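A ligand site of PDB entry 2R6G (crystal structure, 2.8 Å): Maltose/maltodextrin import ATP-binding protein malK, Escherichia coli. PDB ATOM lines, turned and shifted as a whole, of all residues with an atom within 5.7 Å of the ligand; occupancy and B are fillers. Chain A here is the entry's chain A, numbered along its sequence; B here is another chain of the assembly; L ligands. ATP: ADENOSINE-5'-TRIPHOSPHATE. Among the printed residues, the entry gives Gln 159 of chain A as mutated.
The guanidinium group of Arg 129 of chain B is in hydrogen-bond range of the backbone carbonyl oxygen of Ala 133 of chain B, 2.9 Å away.
ND1 of His 192 lies close to O of Gly 36.
The side-chain amide oxygen (OE1) of Gln 82 lies within hydrogen-bond range of the side-chain amide nitrogen (NE2) of Gln 159, 3.0 Å away.
NE2 of Gln 82 sits at hydrogen-bond distance from OG of Ser 43.
The side-chain amide oxygen (OE1) of Gln 82 sits at hydrogen-bond distance from the side-chain amide nitrogen (ND2) of Asn 163 of chain B, 3.4 Å away.
SG of Cys 40 sits close to NZ of Lys 42 (3.6 Å).
NZ of Lys 42 is in hydrogen-bond range of O of Pro 37.
The backbone carbonyl oxygen (O) of Gly 36 is in hydrogen-bond range of the side-chain amino group (NZ) of Lys 42, 2.9 Å away.
Merely in contact with the ligand: Trp 13 (3.6 Å), Val 18 (3.3 Å), Pro 37 (3.9 Å) and Ala 133 of chain B (3.3 Å).
Hydrophobic or aromatic side chains that line the ligand: Trp 13, Val 18, His 192 and Ala 133 of chain B.
The backbone NH (N) of Thr 44 lies within hydrogen-bond range of an oxygen (O2A) of the ligand.
The side-chain hydroxyl (OG1) of Thr 44 sits at hydrogen-bond distance from an oxygen (O2A) of the ligand.
NH1 of Arg 129 of chain B lies within hydrogen-bond range of O2' of the ligand (2.6 Å).
The side-chain hydroxyl (OG) of Ser 135 of chain B sits at hydrogen-bond distance from an oxygen (O1G) of the ligand (2.6 Å).
O1G of the ligand lies within hydrogen-bond range of N of Gly 39 (2.7 Å).
O3' of the ligand is in hydrogen-bond range of O of Gly 39 (2.7 Å).
N of Gly 137 of chain B sits at hydrogen-bond distance from O3G of the ligand.
OE1 of Gln 138 of chain B lies within hydrogen-bond range of O2' of the ligand (2.7 Å).
NE2 of His 192 lies within hydrogen-bond range of O2G of the ligand (2.8 Å).
O3G of the ligand sits close to OE1 of Gln 82 (2.8 Å).
The backbone NH of Lys 42 is in hydrogen-bond range of an oxygen (O2B) of the ligand (2.9 Å).
The side-chain amino group (NZ) of Lys 42 lies within salt-bridge range of an oxygen (O2B) of the ligand (2.8 Å).
The side-chain amide nitrogen (NE2) of Gln 159 is in hydrogen-bond range of an oxygen (O2G) of the ligand.
The side-chain hydroxyl (OG) of Ser 38 is in hydrogen-bond range of an oxygen (O1G) of the ligand.
N of Ser 43 lies within hydrogen-bond range of O3A of the ligand, 3.0 Å away.
O3G of the ligand is in hydrogen-bond range of N of Gly 136 of chain B (3.2 Å).
The backbone NH (N) of Gly 41 sits at hydrogen-bond distance from an oxygen (O2B) of the ligand.
The side-chain sulfur of Cys 40 is in hydrogen-bond range of an oxygen (O2B) of the ligand, at 3.5 Å.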
ATOM      1  N   TRP A  13      17.693 -25.449   1.252  1.00  0.00           N
ATOM      2  CA  TRP A  13      17.781 -25.073   2.665  1.00  0.00           C
ATOM      3  C   TRP A  13      19.033 -25.723   3.246  1.00  0.00           C
ATOM      4  O   TRP A  13      18.955 -26.646   4.076  1.00  0.00           O
ATOM      5  CB  TRP A  13      16.522 -25.482   3.423  1.00  0.00           C
ATOM      6  CG  TRP A  13      15.252 -24.931   2.835  1.00  0.00           C
ATOM      7  CD1 TRP A  13      14.395 -25.579   1.984  1.00  0.00           C
ATOM      8  CD2 TRP A  13      14.692 -23.630   3.054  1.00  0.00           C
ATOM      9  NE1 TRP A  13      13.338 -24.760   1.660  1.00  0.00           N
ATOM     10  CE2 TRP A  13      13.499 -23.550   2.303  1.00  0.00           C
ATOM     11  CE3 TRP A  13      15.099 -22.511   3.804  1.00  0.00           C
ATOM     12  CZ2 TRP A  13      12.697 -22.409   2.281  1.00  0.00           C
ATOM     13  CZ3 TRP A  13      14.294 -21.369   3.792  1.00  0.00           C
ATOM     14  CH2 TRP A  13      13.108 -21.332   3.026  1.00  0.00           C
ATOM     15  N   VAL A  16      19.044 -29.696   2.335  1.00  0.00           N
ATOM     16  CA  VAL A  16      17.757 -30.093   1.735  1.00  0.00           C
ATOM     17  C   VAL A  16      17.461 -29.275   0.482  1.00  0.00           C
ATOM     18  O   VAL A  16      17.199 -28.073   0.551  1.00  0.00           O
ATOM     19  CB  VAL A  16      16.589 -29.972   2.767  1.00  0.00           C
ATOM     20  CG1 VAL A  16      15.241 -30.245   2.105  1.00  0.00           C
ATOM     21  CG2 VAL A  16      16.821 -30.910   3.947  1.00  0.00           C
ATOM     22  N   VAL A  18      14.852 -28.785  -2.310  1.00  0.00           N
ATOM     23  CA  VAL A  18      13.465 -29.083  -2.677  1.00  0.00           C
ATOM     24  C   VAL A  18      13.018 -28.408  -3.985  1.00  0.00           C
ATOM     25  O   VAL A  18      11.826 -28.379  -4.321  1.00  0.00           O
ATOM     26  CB  VAL A  18      12.486 -28.793  -1.497  1.00  0.00           C
ATOM     27  CG1 VAL A  18      12.233 -27.293  -1.336  1.00  0.00           C
ATOM     28  CG2 VAL A  18      11.178 -29.574  -1.688  1.00  0.00           C
ATOM     29  N   GLY A  36       1.071 -31.739  -7.761  1.00  0.00           N
ATOM     30  CA  GLY A  36       2.231 -32.442  -7.226  1.00  0.00           C
ATOM     31  C   GLY A  36       1.960 -32.962  -5.831  1.00  0.00           C
ATOM     32  O   GLY A  36       1.081 -32.450  -5.134  1.00  0.00           O
ATOM     33  N   PRO A  37       2.724 -33.992  -5.400  1.00  0.00           N
ATOM     34  CA  PRO A  37       2.514 -34.619  -4.093  1.00  0.00           C
ATOM     35  C   PRO A  37       2.748 -33.626  -2.964  1.00  0.00           C
ATOM     36  O   PRO A  37       3.511 -32.678  -3.128  1.00  0.00           O
ATOM     37  CB  PRO A  37       3.579 -35.713  -4.056  1.00  0.00           C
ATOM     38  CG  PRO A  37       3.956 -35.952  -5.462  1.00  0.00           C
ATOM     39  CD  PRO A  37       3.838 -34.615  -6.129  1.00  0.00           C
ATOM     40  N   SER A  38       2.090 -33.846  -1.835  1.00  0.00           N
ATOM     41  CA  SER A  38       2.352 -33.073  -0.635  1.00  0.00           C
ATOM     42  C   SER A  38       3.849 -33.157  -0.314  1.00  0.00           C
ATOM     43  O   SER A  38       4.381 -34.235  -0.089  1.00  0.00           O
ATOM     44  CB  SER A  38       1.521 -33.581   0.550  1.00  0.00           C
ATOM     45  OG  SER A  38       1.769 -32.826   1.716  1.00  0.00           O
ATOM     46  N   GLY A  39       4.524 -32.002  -0.346  1.00  0.00           N
ATOM     47  CA  GLY A  39       5.947 -31.949  -0.040  1.00  0.00           C
ATOM     48  C   GLY A  39       6.867 -31.663  -1.209  1.00  0.00           C
ATOM     49  O   GLY A  39       8.052 -31.418  -1.006  1.00  0.00           O
ATOM     50  N   CYS A  40       6.324 -31.692  -2.429  1.00  0.00           N
ATOM     51  CA  CYS A  40       7.139 -31.580  -3.646  1.00  0.00           C
ATOM     52  C   CYS A  40       7.797 -30.211  -3.850  1.00  0.00           C
ATOM     53  O   CYS A  40       8.876 -30.119  -4.456  1.00  0.00           O
ATOM     54  CB  CYS A  40       6.324 -31.971  -4.887  1.00  0.00           C
ATOM     55  SG  CYS A  40       4.941 -30.860  -5.278  1.00  0.00           S
ATOM     56  N   GLY A  41       7.164 -29.154  -3.337  1.00  0.00           N
ATOM     57  CA  GLY A  41       7.727 -27.812  -3.401  1.00  0.00           C
ATOM     58  C   GLY A  41       6.919 -26.845  -4.250  1.00  0.00           C
ATOM     59  O   GLY A  41       7.487 -25.991  -4.919  1.00  0.00           O
ATOM     60  N   LYS A  42       5.597 -26.982  -4.200  1.00  0.00           N
ATOM     61  CA  LYS A  42       4.693 -26.115  -4.955  1.00  0.00           C
ATOM     62  C   LYS A  42       4.665 -24.713  -4.368  1.00  0.00           C
ATOM     63  O   LYS A  42       4.826 -23.734  -5.092  1.00  0.00           O
ATOM     64  CB  LYS A  42       3.277 -26.695  -4.989  1.00  0.00           C
ATOM     65  CG  LYS A  42       3.157 -28.047  -5.679  1.00  0.00           C
ATOM     66  CD  LYS A  42       1.730 -28.573  -5.680  1.00  0.00           C
ATOM     67  CE  LYS A  42       1.215 -28.857  -4.279  1.00  0.00           C
ATOM     68  NZ  LYS A  42       1.830 -30.076  -3.678  1.00  0.00           N
ATOM     69  N   SER A  43       4.456 -24.635  -3.051  1.00  0.00           N
ATOM     70  CA  SER A  43       4.377 -23.352  -2.353  1.00  0.00           C
ATOM     71  C   SER A  43       5.684 -22.570  -2.510  1.00  0.00           C
ATOM     72  O   SER A  43       5.659 -21.353  -2.725  1.00  0.00           O
ATOM     73  CB  SER A  43       4.035 -23.558  -0.874  1.00  0.00           C
ATOM     74  OG  SER A  43       2.785 -24.229  -0.721  1.00  0.00           O
ATOM     75  N   THR A  44       6.808 -23.276  -2.417  1.00  0.00           N
ATOM     76  CA  THR A  44       8.129 -22.671  -2.562  1.00  0.00           C
ATOM     77  C   THR A  44       8.251 -21.934  -3.897  1.00  0.00           C
ATOM     78  O   THR A  44       8.659 -20.774  -3.929  1.00  0.00           O
ATOM     79  CB  THR A  44       9.247 -23.723  -2.439  1.00  0.00           C
ATOM     80  OG1 THR A  44       9.099 -24.426  -1.200  1.00  0.00           O
ATOM     81  CG2 THR A  44      10.623 -23.075  -2.466  1.00  0.00           C
ATOM     82  N   LEU A  45       7.890 -22.632  -4.978  1.00  0.00           N
ATOM     83  CA  LEU A  45       7.918 -22.049  -6.317  1.00  0.00           C
ATOM     84  C   LEU A  45       7.178 -20.726  -6.315  1.00  0.00           C
ATOM     85  O   LEU A  45       7.742 -19.701  -6.706  1.00  0.00           O
ATOM     86  CB  LEU A  45       7.321 -22.993  -7.354  1.00  0.00           C
ATOM     87  CG  LEU A  45       8.034 -24.299  -7.714  1.00  0.00           C
ATOM     88  CD1 LEU A  45       7.449 -24.852  -9.004  1.00  0.00           C
ATOM     89  CD2 LEU A  45       9.540 -24.131  -7.845  1.00  0.00           C
ATOM     90  N   GLN A  82      -1.576 -20.425   1.059  1.00  0.00           N
ATOM     91  CA  GLN A  82      -2.053 -21.755   1.453  1.00  0.00           C
ATOM     92  C   GLN A  82      -2.467 -21.762   2.913  1.00  0.00           C
ATOM     93  O   GLN A  82      -3.438 -22.436   3.291  1.00  0.00           O
ATOM     94  CB  GLN A  82      -0.980 -22.828   1.185  1.00  0.00           C
ATOM     95  CG  GLN A  82      -1.214 -24.150   1.918  1.00  0.00           C
ATOM     96  CD  GLN A  82      -0.620 -25.338   1.216  1.00  0.00           C
ATOM     97  OE1 GLN A  82      -0.837 -26.477   1.622  1.00  0.00           O
ATOM     98  NE2 GLN A  82       0.148 -25.099   0.151  1.00  0.00           N
ATOM     99  N   GLN A 159      -3.623 -23.396  -3.277  1.00  0.00           N
ATOM    100  CA  GLN A 159      -4.695 -24.259  -2.745  1.00  0.00           C
ATOM    101  C   GLN A 159      -5.878 -23.482  -2.168  1.00  0.00           C
ATOM    102  O   GLN A 159      -6.218 -23.655  -0.996  1.00  0.00           O
ATOM    103  CB  GLN A 159      -4.124 -25.222  -1.697  1.00  0.00           C
ATOM    104  CG  GLN A 159      -3.013 -26.126  -2.200  1.00  0.00           C
ATOM    105  CD  GLN A 159      -2.694 -27.242  -1.228  1.00  0.00           C
ATOM    106  OE1 GLN A 159      -3.590 -27.792  -0.585  1.00  0.00           O
ATOM    107  NE2 GLN A 159      -1.414 -27.593  -1.129  1.00  0.00           N
ATOM    108  N   HIS A 192      -4.787 -29.430  -5.303  1.00  0.00           N
ATOM    109  CA  HIS A 192      -4.674 -30.883  -5.207  1.00  0.00           C
ATOM    110  C   HIS A 192      -5.891 -31.542  -5.855  1.00  0.00           C
ATOM    111  O   HIS A 192      -5.841 -32.727  -6.213  1.00  0.00           O
ATOM    112  CB  HIS A 192      -4.532 -31.335  -3.752  1.00  0.00           C
ATOM    113  CG  HIS A 192      -3.150 -31.174  -3.195  1.00  0.00           C
ATOM    114  ND1 HIS A 192      -2.044 -31.811  -3.714  1.00  0.00           N
ATOM    115  CD2 HIS A 192      -2.698 -30.445  -2.142  1.00  0.00           C
ATOM    116  CE1 HIS A 192      -0.975 -31.488  -3.019  1.00  0.00           C
ATOM    117  NE2 HIS A 192      -1.343 -30.659  -2.054  1.00  0.00           N
ATOM    118  N   LEU B 126      10.741 -36.784   8.421  1.00  0.00           N
ATOM    119  CA  LEU B 126      10.521 -35.426   8.910  1.00  0.00           C
ATOM    120  C   LEU B 126      10.398 -35.391  10.426  1.00  0.00           C
ATOM    121  O   LEU B 126       9.909 -34.423  11.003  1.00  0.00           O
ATOM    122  CB  LEU B 126       9.262 -34.838   8.280  1.00  0.00           C
ATOM    123  CG  LEU B 126       9.164 -34.816   6.753  1.00  0.00           C
ATOM    124  CD1 LEU B 126       7.771 -34.388   6.328  1.00  0.00           C
ATOM    125  CD2 LEU B 126      10.231 -33.913   6.131  1.00  0.00           C
ATOM    126  N   ARG B 129      12.114 -32.496  12.265  1.00  0.00           N
ATOM    127  CA  ARG B 129      11.713 -31.187  11.754  1.00  0.00           C
ATOM    128  C   ARG B 129      10.834 -30.453  12.746  1.00  0.00           C
ATOM    129  O   ARG B 129       9.925 -31.032  13.345  1.00  0.00           O
ATOM    130  CB  ARG B 129      10.965 -31.339  10.428  1.00  0.00           C
ATOM    131  CG  ARG B 129      11.830 -31.676   9.237  1.00  0.00           C
ATOM    132  CD  ARG B 129      12.294 -30.413   8.518  1.00  0.00           C
ATOM    133  NE  ARG B 129      12.852 -30.719   7.207  1.00  0.00           N
ATOM    134  CZ  ARG B 129      12.144 -30.813   6.087  1.00  0.00           C
ATOM    135  NH1 ARG B 129      10.836 -30.606   6.109  1.00  0.00           N
ATOM    136  NH2 ARG B 129      12.738 -31.102   4.933  1.00  0.00           N
ATOM    137  N   LYS B 132       7.492 -25.083  11.490  1.00  0.00           N
ATOM    138  CA  LYS B 132       7.633 -24.014  10.498  1.00  0.00           C
ATOM    139  C   LYS B 132       8.580 -24.378   9.336  1.00  0.00           C
ATOM    140  O   LYS B 132       8.691 -23.629   8.365  1.00  0.00           O
ATOM    141  CB  LYS B 132       8.039 -22.682  11.155  1.00  0.00           C
ATOM    142  CG  LYS B 132       9.483 -22.608  11.634  1.00  0.00           C
ATOM    143  CD  LYS B 132       9.902 -21.157  11.842  1.00  0.00           C
ATOM    144  CE  LYS B 132      11.354 -21.034  12.298  1.00  0.00           C
ATOM    145  NZ  LYS B 132      11.532 -21.496  13.702  1.00  0.00           N
ATOM    146  N   ALA B 133       9.232 -25.526   9.448  1.00  0.00           N
ATOM    147  CA  ALA B 133      10.090 -26.053   8.388  1.00  0.00           C
ATOM    148  C   ALA B 133       9.407 -27.176   7.593  1.00  0.00           C
ATOM    149  O   ALA B 133      10.063 -27.967   6.915  1.00  0.00           O
ATOM    150  CB  ALA B 133      11.416 -26.524   8.954  1.00  0.00           C
ATOM    151  N   LEU B 134       8.081 -27.230   7.676  1.00  0.00           N
ATOM    152  CA  LEU B 134       7.279 -28.214   6.936  1.00  0.00           C
ATOM    153  C   LEU B 134       6.446 -27.555   5.844  1.00  0.00           C
ATOM    154  O   LEU B 134       6.468 -26.336   5.685  1.00  0.00           O
ATOM    155  CB  LEU B 134       6.352 -28.984   7.894  1.00  0.00           C
ATOM    156  CG  LEU B 134       6.942 -29.827   9.022  1.00  0.00           C
ATOM    157  CD1 LEU B 134       5.815 -30.259   9.949  1.00  0.00           C
ATOM    158  CD2 LEU B 134       7.722 -31.029   8.494  1.00  0.00           C
ATOM    159  N   SER B 135       5.710 -28.379   5.100  1.00  0.00           N
ATOM    160  CA  SER B 135       4.753 -27.895   4.112  1.00  0.00           C
ATOM    161  C   SER B 135       3.349 -27.950   4.686  1.00  0.00           C
ATOM    162  O   SER B 135       3.097 -28.659   5.651  1.00  0.00           O
ATOM    163  CB  SER B 135       4.831 -28.742   2.847  1.00  0.00           C
ATOM    164  OG  SER B 135       3.913 -29.825   2.880  1.00  0.00           O
ATOM    165  N   GLY B 136       2.427 -27.188   4.083  1.00  0.00           N
ATOM    166  CA  GLY B 136       1.039 -27.147   4.537  1.00  0.00           C
ATOM    167  C   GLY B 136       0.436 -28.516   4.769  1.00  0.00           C
ATOM    168  O   GLY B 136      -0.089 -28.796   5.851  1.00  0.00           O
ATOM    169  N   GLY B 137       0.543 -29.384   3.757  1.00  0.00           N
ATOM    170  CA  GLY B 137       0.016 -30.742   3.833  1.00  0.00           C
ATOM    171  C   GLY B 137       0.767 -31.644   4.795  1.00  0.00           C
ATOM    172  O   GLY B 137       0.178 -32.535   5.408  1.00  0.00           O
ATOM    173  N   GLN B 138       2.069 -31.394   4.940  1.00  0.00           N
ATOM    174  CA  GLN B 138       2.906 -32.151   5.863  1.00  0.00           C
ATOM    175  C   GLN B 138       2.527 -31.890   7.319  1.00  0.00           C
ATOM    176  O   GLN B 138       2.528 -32.809   8.141  1.00  0.00           O
ATOM    177  CB  GLN B 138       4.381 -31.837   5.624  1.00  0.00           C
ATOM    178  CG  GLN B 138       4.923 -32.445   4.336  1.00  0.00           C
ATOM    179  CD  GLN B 138       6.353 -32.051   4.054  1.00  0.00           C
ATOM    180  OE1 GLN B 138       6.828 -31.014   4.518  1.00  0.00           O
ATOM    181  NE2 GLN B 138       7.058 -32.884   3.301  1.00  0.00           N
ATOM    182  N   ASN B 163      -5.768 -30.645   2.468  1.00  0.00           N
ATOM    183  CA  ASN B 163      -4.592 -30.156   1.750  1.00  0.00           C
ATOM    184  C   ASN B 163      -3.601 -31.266   1.386  1.00  0.00           C
ATOM    185  O   ASN B 163      -2.393 -31.139   1.576  1.00  0.00           O
ATOM    186  CB  ASN B 163      -3.905 -29.044   2.558  1.00  0.00           C
ATOM    187  CG  ASN B 163      -4.735 -27.762   2.609  1.00  0.00           C
ATOM    188  OD1 ASN B 163      -5.791 -27.715   3.262  1.00  0.00           O
ATOM    189  ND2 ASN B 163      -4.263 -26.724   1.924  1.00  0.00           N
HETATM  190  PG  ATP L   1       1.869 -29.053   0.176  1.00  0.00           P
HETATM  191  O1G ATP L   1       2.719 -30.235   0.574  1.00  0.00           O
HETATM  192  O2G ATP L   1       0.888 -29.395  -0.922  1.00  0.00           O
HETATM  193  O3G ATP L   1       1.276 -28.314   1.342  1.00  0.00           O
HETATM  194  PB  ATP L   1       4.296 -28.323  -1.086  1.00  0.00           P
HETATM  195  O1B ATP L   1       5.037 -29.170  -0.090  1.00  0.00           O
HETATM  196  O2B ATP L   1       4.107 -28.851  -2.485  1.00  0.00           O
HETATM  197  O3B ATP L   1       2.856 -27.950  -0.468  1.00  0.00           O
HETATM  198  PA  ATP L   1       6.193 -26.481  -0.113  1.00  0.00           P
HETATM  199  O1A ATP L   1       5.598 -26.411   1.262  1.00  0.00           O
HETATM  200  O2A ATP L   1       6.872 -25.259  -0.665  1.00  0.00           O
HETATM  201  O3A ATP L   1       5.051 -26.910  -1.169  1.00  0.00           O
HETATM  202  O5' ATP L   1       7.269 -27.681  -0.147  1.00  0.00           O
HETATM  203  C5' ATP L   1       8.529 -27.462   0.492  1.00  0.00           C
HETATM  204  C4' ATP L   1       9.181 -28.786   0.884  1.00  0.00           C
HETATM  205  O4' ATP L   1      10.494 -28.541   1.379  1.00  0.00           O
HETATM  206  C3' ATP L   1       8.418 -29.516   1.985  1.00  0.00           C
HETATM  207  O3' ATP L   1       8.305 -30.892   1.614  1.00  0.00           O
HETATM  208  C2' ATP L   1       9.271 -29.388   3.241  1.00  0.00           C
HETATM  209  O2' ATP L   1       9.472 -30.652   3.864  1.00  0.00           O
HETATM  210  C1' ATP L   1      10.593 -28.811   2.783  1.00  0.00           C
HETATM  211  N9  ATP L   1      10.834 -27.545   3.509  1.00  0.00           N
HETATM  212  C8  ATP L   1      10.021 -26.471   3.543  1.00  0.00           C
HETATM  213  N7  ATP L   1      10.535 -25.476   4.317  1.00  0.00           N
HETATM  214  C5  ATP L   1      11.717 -25.920   4.783  1.00  0.00           C
HETATM  215  C6  ATP L   1      12.794 -25.379   5.650  1.00  0.00           C
HETATM  216  N6  ATP L   1      12.689 -24.136   6.175  1.00  0.00           N
HETATM  217  N1  ATP L   1      13.859 -26.171   5.901  1.00  0.00           N
HETATM  218  C2  ATP L   1      13.973 -27.415   5.379  1.00  0.00           C
HETATM  219  N3  ATP L   1      13.043 -27.965   4.580  1.00  0.00           N
HETATM  220  C4  ATP L   1      11.915 -27.284   4.256  1.00  0.00           C
